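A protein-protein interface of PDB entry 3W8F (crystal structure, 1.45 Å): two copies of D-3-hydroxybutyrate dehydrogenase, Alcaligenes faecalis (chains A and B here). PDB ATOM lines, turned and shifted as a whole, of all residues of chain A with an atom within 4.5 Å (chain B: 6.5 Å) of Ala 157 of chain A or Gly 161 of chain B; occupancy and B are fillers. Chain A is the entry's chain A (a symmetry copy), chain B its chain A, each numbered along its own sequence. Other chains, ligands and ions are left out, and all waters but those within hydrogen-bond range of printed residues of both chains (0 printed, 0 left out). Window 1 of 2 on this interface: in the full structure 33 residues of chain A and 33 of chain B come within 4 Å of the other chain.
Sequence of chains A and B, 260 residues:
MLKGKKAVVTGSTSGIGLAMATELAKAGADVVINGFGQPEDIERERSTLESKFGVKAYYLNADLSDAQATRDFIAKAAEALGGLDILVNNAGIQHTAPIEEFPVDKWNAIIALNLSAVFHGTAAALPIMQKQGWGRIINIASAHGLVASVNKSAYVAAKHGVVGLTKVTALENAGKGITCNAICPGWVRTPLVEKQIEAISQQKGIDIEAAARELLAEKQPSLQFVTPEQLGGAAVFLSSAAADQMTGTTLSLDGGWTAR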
ATOM      1  N   TRP A 107       0.376  17.967 -21.444  1.00  0.00           N
ATOM      2  CA  TRP A 107       0.377  16.496 -21.656  1.00  0.00           C
ATOM      3  C   TRP A 107       1.497  15.875 -20.885  1.00  0.00           C
ATOM      4  O   TRP A 107       1.247  14.937 -20.143  1.00  0.00           O
ATOM      5  CB  TRP A 107       0.492  16.216 -23.171  1.00  0.00           C
ATOM      6  CG  TRP A 107       0.729  14.787 -23.449  1.00  0.00           C
ATOM      7  CD1 TRP A 107       1.935  14.153 -23.522  1.00  0.00           C
ATOM      8  CD2 TRP A 107      -0.261  13.773 -23.684  1.00  0.00           C
ATOM      9  NE1 TRP A 107       1.776  12.797 -23.725  1.00  0.00           N
ATOM     10  CE2 TRP A 107       0.430  12.550 -23.825  1.00  0.00           C
ATOM     11  CE3 TRP A 107      -1.660  13.776 -23.830  1.00  0.00           C
ATOM     12  CZ2 TRP A 107      -0.220  11.308 -24.053  1.00  0.00           C
ATOM     13  CZ3 TRP A 107      -2.300  12.474 -24.037  1.00  0.00           C
ATOM     14  CH2 TRP A 107      -1.532  11.305 -24.124  1.00  0.00           C
ATOM     15  N   SER A 153      -7.963  14.893 -22.940  1.00  0.00           N
ATOM     16  CA  SER A 153      -7.125  13.842 -23.526  1.00  0.00           C
ATOM     17  C   SER A 153      -6.056  13.298 -22.601  1.00  0.00           C
ATOM     18  O   SER A 153      -5.902  12.088 -22.393  1.00  0.00           O
ATOM     19  CB  SER A 153      -6.520  14.269 -24.855  1.00  0.00           C
ATOM     20  OG  SER A 153      -5.754  15.508 -24.676  1.00  0.00           O
ATOM     21  N   ALA A 154      -5.207  14.183 -22.053  1.00  0.00           N
ATOM     22  CA  ALA A 154      -4.127  13.692 -21.234  1.00  0.00           C
ATOM     23  C   ALA A 154      -4.620  12.983 -19.989  1.00  0.00           C
ATOM     24  O   ALA A 154      -4.035  11.962 -19.598  1.00  0.00           O
ATOM     25  CB  ALA A 154      -3.153  14.892 -20.891  1.00  0.00           C
ATOM     26  N   TYR A 155      -5.605  13.599 -19.338  1.00  0.00           N
ATOM     27  CA  TYR A 155      -6.045  13.024 -18.090  1.00  0.00           C
ATOM     28  C   TYR A 155      -6.794  11.662 -18.285  1.00  0.00           C
ATOM     29  O   TYR A 155      -6.516  10.741 -17.550  1.00  0.00           O
ATOM     30  CB  TYR A 155      -7.047  14.032 -17.498  1.00  0.00           C
ATOM     31  CG  TYR A 155      -7.588  13.714 -16.100  1.00  0.00           C
ATOM     32  CD1 TYR A 155      -6.897  14.149 -15.000  1.00  0.00           C
ATOM     33  CD2 TYR A 155      -8.795  13.029 -15.941  1.00  0.00           C
ATOM     34  CE1 TYR A 155      -7.404  13.980 -13.703  1.00  0.00           C
ATOM     35  CE2 TYR A 155      -9.273  12.797 -14.659  1.00  0.00           C
ATOM     36  CZ  TYR A 155      -8.609  13.313 -13.581  1.00  0.00           C
ATOM     37  OH  TYR A 155      -9.111  13.139 -12.322  1.00  0.00           O
ATOM     38  N   VAL A 156      -7.607  11.581 -19.312  1.00  0.00           N
ATOM     39  CA  VAL A 156      -8.260  10.294 -19.613  1.00  0.00           C
ATOM     40  C   VAL A 156      -7.265   9.276 -19.991  1.00  0.00           C
ATOM     41  O   VAL A 156      -7.310   8.105 -19.543  1.00  0.00           O
ATOM     42  CB  VAL A 156      -9.328  10.495 -20.716  1.00  0.00           C
ATOM     43  CG1 VAL A 156      -9.881   9.130 -21.172  1.00  0.00           C
ATOM     44  CG2 VAL A 156     -10.437  11.312 -20.211  1.00  0.00           C
ATOM     45  N   ALA A 157      -6.248   9.624 -20.834  1.00  0.00           N
ATOM     46  CA  ALA A 157      -5.200   8.685 -21.187  1.00  0.00           C
ATOM     47  C   ALA A 157      -4.474   8.226 -19.921  1.00  0.00           C
ATOM     48  O   ALA A 157      -4.226   7.005 -19.727  1.00  0.00           O
ATOM     49  CB  ALA A 157      -4.229   9.314 -22.190  1.00  0.00           C
ATOM     50  N   ALA A 158      -4.065   9.184 -19.069  1.00  0.00           N
ATOM     51  CA  ALA A 158      -3.346   8.778 -17.893  1.00  0.00           C
ATOM     52  C   ALA A 158      -4.128   7.880 -16.953  1.00  0.00           C
ATOM     53  O   ALA A 158      -3.606   6.928 -16.432  1.00  0.00           O
ATOM     54  CB  ALA A 158      -2.940  10.064 -17.120  1.00  0.00           C
ATOM     55  N   LYS A 159      -5.432   8.230 -16.756  1.00  0.00           N
ATOM     56  CA  LYS A 159      -6.253   7.463 -15.834  1.00  0.00           C
ATOM     57  C   LYS A 159      -6.582   6.085 -16.385  1.00  0.00           C
ATOM     58  O   LYS A 159      -6.595   5.110 -15.624  1.00  0.00           O
ATOM     59  CB  LYS A 159      -7.566   8.225 -15.447  1.00  0.00           C
ATOM     60  CG  LYS A 159      -7.300   9.521 -14.697  1.00  0.00           C
ATOM     61  CD  LYS A 159      -6.638   9.221 -13.319  1.00  0.00           C
ATOM     62  CE  LYS A 159      -6.718  10.504 -12.419  1.00  0.00           C
ATOM     63  NZ  LYS A 159      -6.054  10.185 -11.141  1.00  0.00           N
ATOM     64  N   HIS A 160      -6.812   5.968 -17.701  1.00  0.00           N
ATOM     65  CA  HIS A 160      -6.926   4.631 -18.299  1.00  0.00           C
ATOM     66  C   HIS A 160      -5.631   3.902 -18.065  1.00  0.00           C
ATOM     67  O   HIS A 160      -5.643   2.709 -17.701  1.00  0.00           O
ATOM     68  CB  HIS A 160      -7.181   4.737 -19.801  1.00  0.00           C
ATOM     69  CG  HIS A 160      -8.641   4.872 -20.153  1.00  0.00           C
ATOM     70  ND1 HIS A 160      -9.443   5.972 -19.790  1.00  0.00           N
ATOM     71  CD2 HIS A 160      -9.451   4.033 -20.862  1.00  0.00           C
ATOM     72  CE1 HIS A 160     -10.691   5.743 -20.257  1.00  0.00           C
ATOM     73  NE2 HIS A 160     -10.704   4.597 -20.907  1.00  0.00           N
ATOM     74  N   GLY A 161      -4.465   4.573 -18.215  1.00  0.00           N
ATOM     75  CA  GLY A 161      -3.185   3.949 -17.933  1.00  0.00           C
ATOM     76  C   GLY A 161      -3.050   3.443 -16.546  1.00  0.00           C
ATOM     77  O   GLY A 161      -2.523   2.342 -16.333  1.00  0.00           O
ATOM     78  N   LEU B 115       2.165   5.656 -26.476  1.00  0.00           N
ATOM     79  CA  LEU B 115       1.059   6.513 -26.048  1.00  0.00           C
ATOM     80  C   LEU B 115       1.264   7.914 -26.543  1.00  0.00           C
ATOM     81  O   LEU B 115       0.421   8.436 -27.262  1.00  0.00           O
ATOM     82  CB  LEU B 115       0.879   6.431 -24.527  1.00  0.00           C
ATOM     83  CG  LEU B 115      -0.169   7.377 -23.929  1.00  0.00           C
ATOM     84  CD1 LEU B 115      -1.569   7.101 -24.572  1.00  0.00           C
ATOM     85  CD2 LEU B 115      -0.179   7.224 -22.432  1.00  0.00           C
ATOM     86  N   GLY B 145      -4.836  -3.193 -24.122  1.00  0.00           N
ATOM     87  CA  GLY B 145      -5.520  -1.945 -23.822  1.00  0.00           C
ATOM     88  C   GLY B 145      -6.819  -2.176 -23.064  1.00  0.00           C
ATOM     89  O   GLY B 145      -7.408  -1.183 -22.651  1.00  0.00           O
ATOM     90  N   VAL B 156       0.984  -2.274 -21.108  1.00  0.00           N
ATOM     91  CA  VAL B 156      -0.444  -2.286 -20.741  1.00  0.00           C
ATOM     92  C   VAL B 156      -0.905  -0.934 -20.381  1.00  0.00           C
ATOM     93  O   VAL B 156      -1.996  -0.473 -20.792  1.00  0.00           O
ATOM     94  CB  VAL B 156      -0.682  -3.302 -19.598  1.00  0.00           C
ATOM     95  CG1 VAL B 156      -2.129  -3.185 -19.078  1.00  0.00           C
ATOM     96  CG2 VAL B 156      -0.457  -4.670 -20.075  1.00  0.00           C
ATOM     97  N   ALA B 157      -0.109  -0.150 -19.594  1.00  0.00           N
ATOM     98  CA  ALA B 157      -0.476   1.213 -19.263  1.00  0.00           C
ATOM     99  C   ALA B 157      -0.627   2.031 -20.547  1.00  0.00           C
ATOM    100  O   ALA B 157      -1.623   2.784 -20.718  1.00  0.00           O
ATOM    101  CB  ALA B 157       0.559   1.837 -18.322  1.00  0.00           C
ATOM    102  N   ALA B 158       0.373   1.953 -21.443  1.00  0.00           N
ATOM    103  CA  ALA B 158       0.271   2.744 -22.639  1.00  0.00           C
ATOM    104  C   ALA B 158      -0.920   2.410 -23.517  1.00  0.00           C
ATOM    105  O   ALA B 158      -1.570   3.282 -24.034  1.00  0.00           O
ATOM    106  CB  ALA B 158       1.568   2.521 -23.465  1.00  0.00           C
ATOM    107  N   LYS B 159      -1.186   1.080 -23.665  1.00  0.00           N
ATOM    108  CA  LYS B 159      -2.277   0.655 -24.526  1.00  0.00           C
ATOM    109  C   LYS B 159      -3.633   0.980 -23.922  1.00  0.00           C
ATOM    110  O   LYS B 159      -4.548   1.376 -24.654  1.00  0.00           O
ATOM    111  CB  LYS B 159      -2.186  -0.871 -24.875  1.00  0.00           C
ATOM    112  CG  LYS B 159      -0.939  -1.222 -25.672  1.00  0.00           C
ATOM    113  CD  LYS B 159      -0.980  -0.536 -27.070  1.00  0.00           C
ATOM    114  CE  LYS B 159       0.095  -1.197 -28.001  1.00  0.00           C
ATOM    115  NZ  LYS B 159       0.042  -0.497 -29.298  1.00  0.00           N
ATOM    116  N   HIS B 160      -3.779   0.862 -22.594  1.00  0.00           N
ATOM    117  CA  HIS B 160      -5.002   1.365 -21.954  1.00  0.00           C
ATOM    118  C   HIS B 160      -5.100   2.841 -22.226  1.00  0.00           C
ATOM    119  O   HIS B 160      -6.192   3.345 -22.556  1.00  0.00           O
ATOM    120  CB  HIS B 160      -4.951   1.132 -20.446  1.00  0.00           C
ATOM    121  CG  HIS B 160      -5.454  -0.229 -20.033  1.00  0.00           C
ATOM    122  ND1 HIS B 160      -4.834  -1.442 -20.389  1.00  0.00           N
ATOM    123  CD2 HIS B 160      -6.530  -0.567 -19.263  1.00  0.00           C
ATOM    124  CE1 HIS B 160      -5.565  -2.449 -19.860  1.00  0.00           C
ATOM    125  NE2 HIS B 160      -6.571  -1.938 -19.179  1.00  0.00           N
ATOM    126  N   GLY B 161      -3.980   3.597 -22.148  1.00  0.00           N
ATOM    127  CA  GLY B 161      -3.992   5.012 -22.470  1.00  0.00           C
ATOM    128  C   GLY B 161      -4.449   5.317 -23.847  1.00  0.00           C
ATOM    129  O   GLY B 161      -5.216   6.268 -24.052  1.00  0.00           O
ATOM    130  N   VAL B 162      -4.026   4.480 -24.821  1.00  0.00           N
ATOM    131  CA  VAL B 162      -4.451   4.681 -26.202  1.00  0.00           C
ATOM    132  C   VAL B 162      -5.949   4.488 -26.310  1.00  0.00           C
ATOM    133  O   VAL B 162      -6.610   5.234 -27.057  1.00  0.00           O
ATOM    134  CB  VAL B 162      -3.722   3.718 -27.119  1.00  0.00           C
ATOM    135  CG1 VAL B 162      -4.335   3.731 -28.549  1.00  0.00           C
ATOM    136  CG2 VAL B 162      -2.257   4.144 -27.230  1.00  0.00           C
ATOM    137  N   VAL B 163      -6.520   3.472 -25.653  1.00  0.00           N
ATOM    138  CA  VAL B 163      -7.975   3.257 -25.705  1.00  0.00           C
ATOM    139  C   VAL B 163      -8.667   4.473 -25.105  1.00  0.00           C
ATOM    140  O   VAL B 163      -9.649   4.967 -25.686  1.00  0.00           O
ATOM    141  CB  VAL B 163      -8.259   1.991 -24.955  1.00  0.00           C
ATOM    142  CG1 VAL B 163      -9.781   1.872 -24.692  1.00  0.00           C
ATOM    143  CG2 VAL B 163      -7.774   0.797 -25.777  1.00  0.00           C
ATOM    144  N   GLY B 164      -8.165   5.056 -24.012  1.00  0.00           N
ATOM    145  CA  GLY B 164      -8.817   6.270 -23.481  1.00  0.00           C
ATOM    146  C   GLY B 164      -8.670   7.438 -24.433  1.00  0.00           C
ATOM    147  O   GLY B 164      -9.661   8.207 -24.625  1.00  0.00           O
ATOM    148  N   LEU B 165      -7.457   7.626 -24.988  1.00  0.00           N
ATOM    149  CA  LEU B 165      -7.279   8.720 -25.905  1.00  0.00           C
ATOM    150  C   LEU B 165      -8.149   8.630 -27.140  1.00  0.00           C
ATOM    151  O   LEU B 165      -8.678   9.645 -27.646  1.00  0.00           O
ATOM    152  CB  LEU B 165      -5.747   8.759 -26.309  1.00  0.00           C
ATOM    153  CG  LEU B 165      -5.364   9.794 -27.292  1.00  0.00           C
ATOM    154  CD1 LEU B 165      -5.588  11.258 -26.734  1.00  0.00           C
ATOM    155  CD2 LEU B 165      -3.894   9.573 -27.522  1.00  0.00           C
ATOM    156  N   THR B 166      -8.382   7.418 -27.630  1.00  0.00           N
ATOM    157  CA  THR B 166      -9.254   7.152 -28.764  1.00  0.00           C
ATOM    158  C   THR B 166     -10.675   7.668 -28.438  1.00  0.00           C
ATOM    159  O   THR B 166     -11.308   8.321 -29.293  1.00  0.00           O
ATOM    160  CB  THR B 166      -9.322   5.638 -28.982  1.00  0.00           C
ATOM    161  OG1 THR B 166      -7.978   5.200 -29.403  1.00  0.00           O
ATOM    162  CG2 THR B 166     -10.328   5.261 -30.083  1.00  0.00           C
ATOM    163  N   VAL B 168     -11.606  10.027 -26.242  1.00  0.00           N
ATOM    164  CA  VAL B 168     -11.611  11.505 -26.224  1.00  0.00           C
ATOM    165  C   VAL B 168     -11.573  12.073 -27.627  1.00  0.00           C
ATOM    166  O   VAL B 168     -12.360  12.964 -27.940  1.00  0.00           O
ATOM    167  CB  VAL B 168     -10.376  12.009 -25.432  1.00  0.00           C
ATOM    168  CG1 VAL B 168     -10.395  13.579 -25.530  1.00  0.00           C
ATOM    169  CG2 VAL B 168     -10.516  11.654 -23.968  1.00  0.00           C
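Of the 14 printed residues of chain B, 7 touch a printed residue of chain A.
Hydrophobic or aromatic side chains of chain B that line the printed part of chain A: Leu 115, Ala 157, His 160, Leu 165 and Val 168.
Printed residues of chain A that touch a printed residue of chain B: Trp 107, Ser 153, Val 156, Ala 157, His 160 and Gly 161.
Hydrophobic or aromatic side chains of chain A within 4 Å of the printed part of chain B: Trp 107, Val 156, Ala 157 and His 160.
Ala 157 of chain A touches just one residue of chain B: Gly 161.
Printed residues of chain A within 4 Å of Gly 161 of chain B: Ala 157.
Of the printed residues of chain B, Ser 153 of chain A touches Leu 165 and Val 168.
Printed residues of chain A within 4 Å of His 160 of chain B: His 160 (3.2 Å).
Of the printed residues of chain B, Gly 161 of chain A touches Ala 157.
Of the printed residues of chain A, Ala 157 of chain B touches Gly 161 (3.4 Å).
Of the printed residues of chain A, Leu 165 of chain B touches Ser 153 (3.7 Å).
The nearest residue of chain B that does not touch Ala 157 of chain A is Leu 115 of chain B (4.2 Å).
The nearest residue of chain A that does not touch Gly 161 of chain B is Gly 161 of chain A (4.1 Å).
O of Val 156 of chain A is in hydrogen-bond range of ND1 of His 160 of chain A (3.0 Å).
O of Gly 145 of chain B lies close to ND1 of His 160 of chain B.
The backbone carbonyl oxygen (O) of Val 156 of chain B is in hydrogen-bond range of a ring nitrogen (ND1) of His 160 of chain B, at 3.0 Å.
CZ2 of Trp 107 of chain A touches CG of Leu 115 of chain B (3.9 Å).
CB of Ser 153 of chain A touches CD1 of Leu 165 of chain B (3.7 Å).
Ser 153 of chain A touches Val 168 of chain B.
Val 156 of chain A touches Gly 164 of chain B.
CB of Val 156 of chain A touches CG2 of Val 168 of chain B, 3.7 Å away.
Gly 161 of chain B touches Ala 157 of chain A (CA to O, 3.4 Å).
His 160 of chain A touches His 160 of chain B.
CD2 of His 160 of chain A touches CA of Gly 164 of chain B, 3.5 Å away.
CA of Gly 161 of chain A touches O of Ala 157 of chain B, 3.4 Å away.
Ala 157 of chain A touches Gly 161 of chain B, and with the chains exchanged Gly 161 of chain A touches Ala 157 of chain B.
His 160 of chain B touches its own counterpart, His 160 of chain A.
Positions printed for both chains: 156, 157, 158, 159, 160 and 161.
Of the 9 pairs that touch across the chains among the printed residues, 3 have their exchanged pair printed and touching as well.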
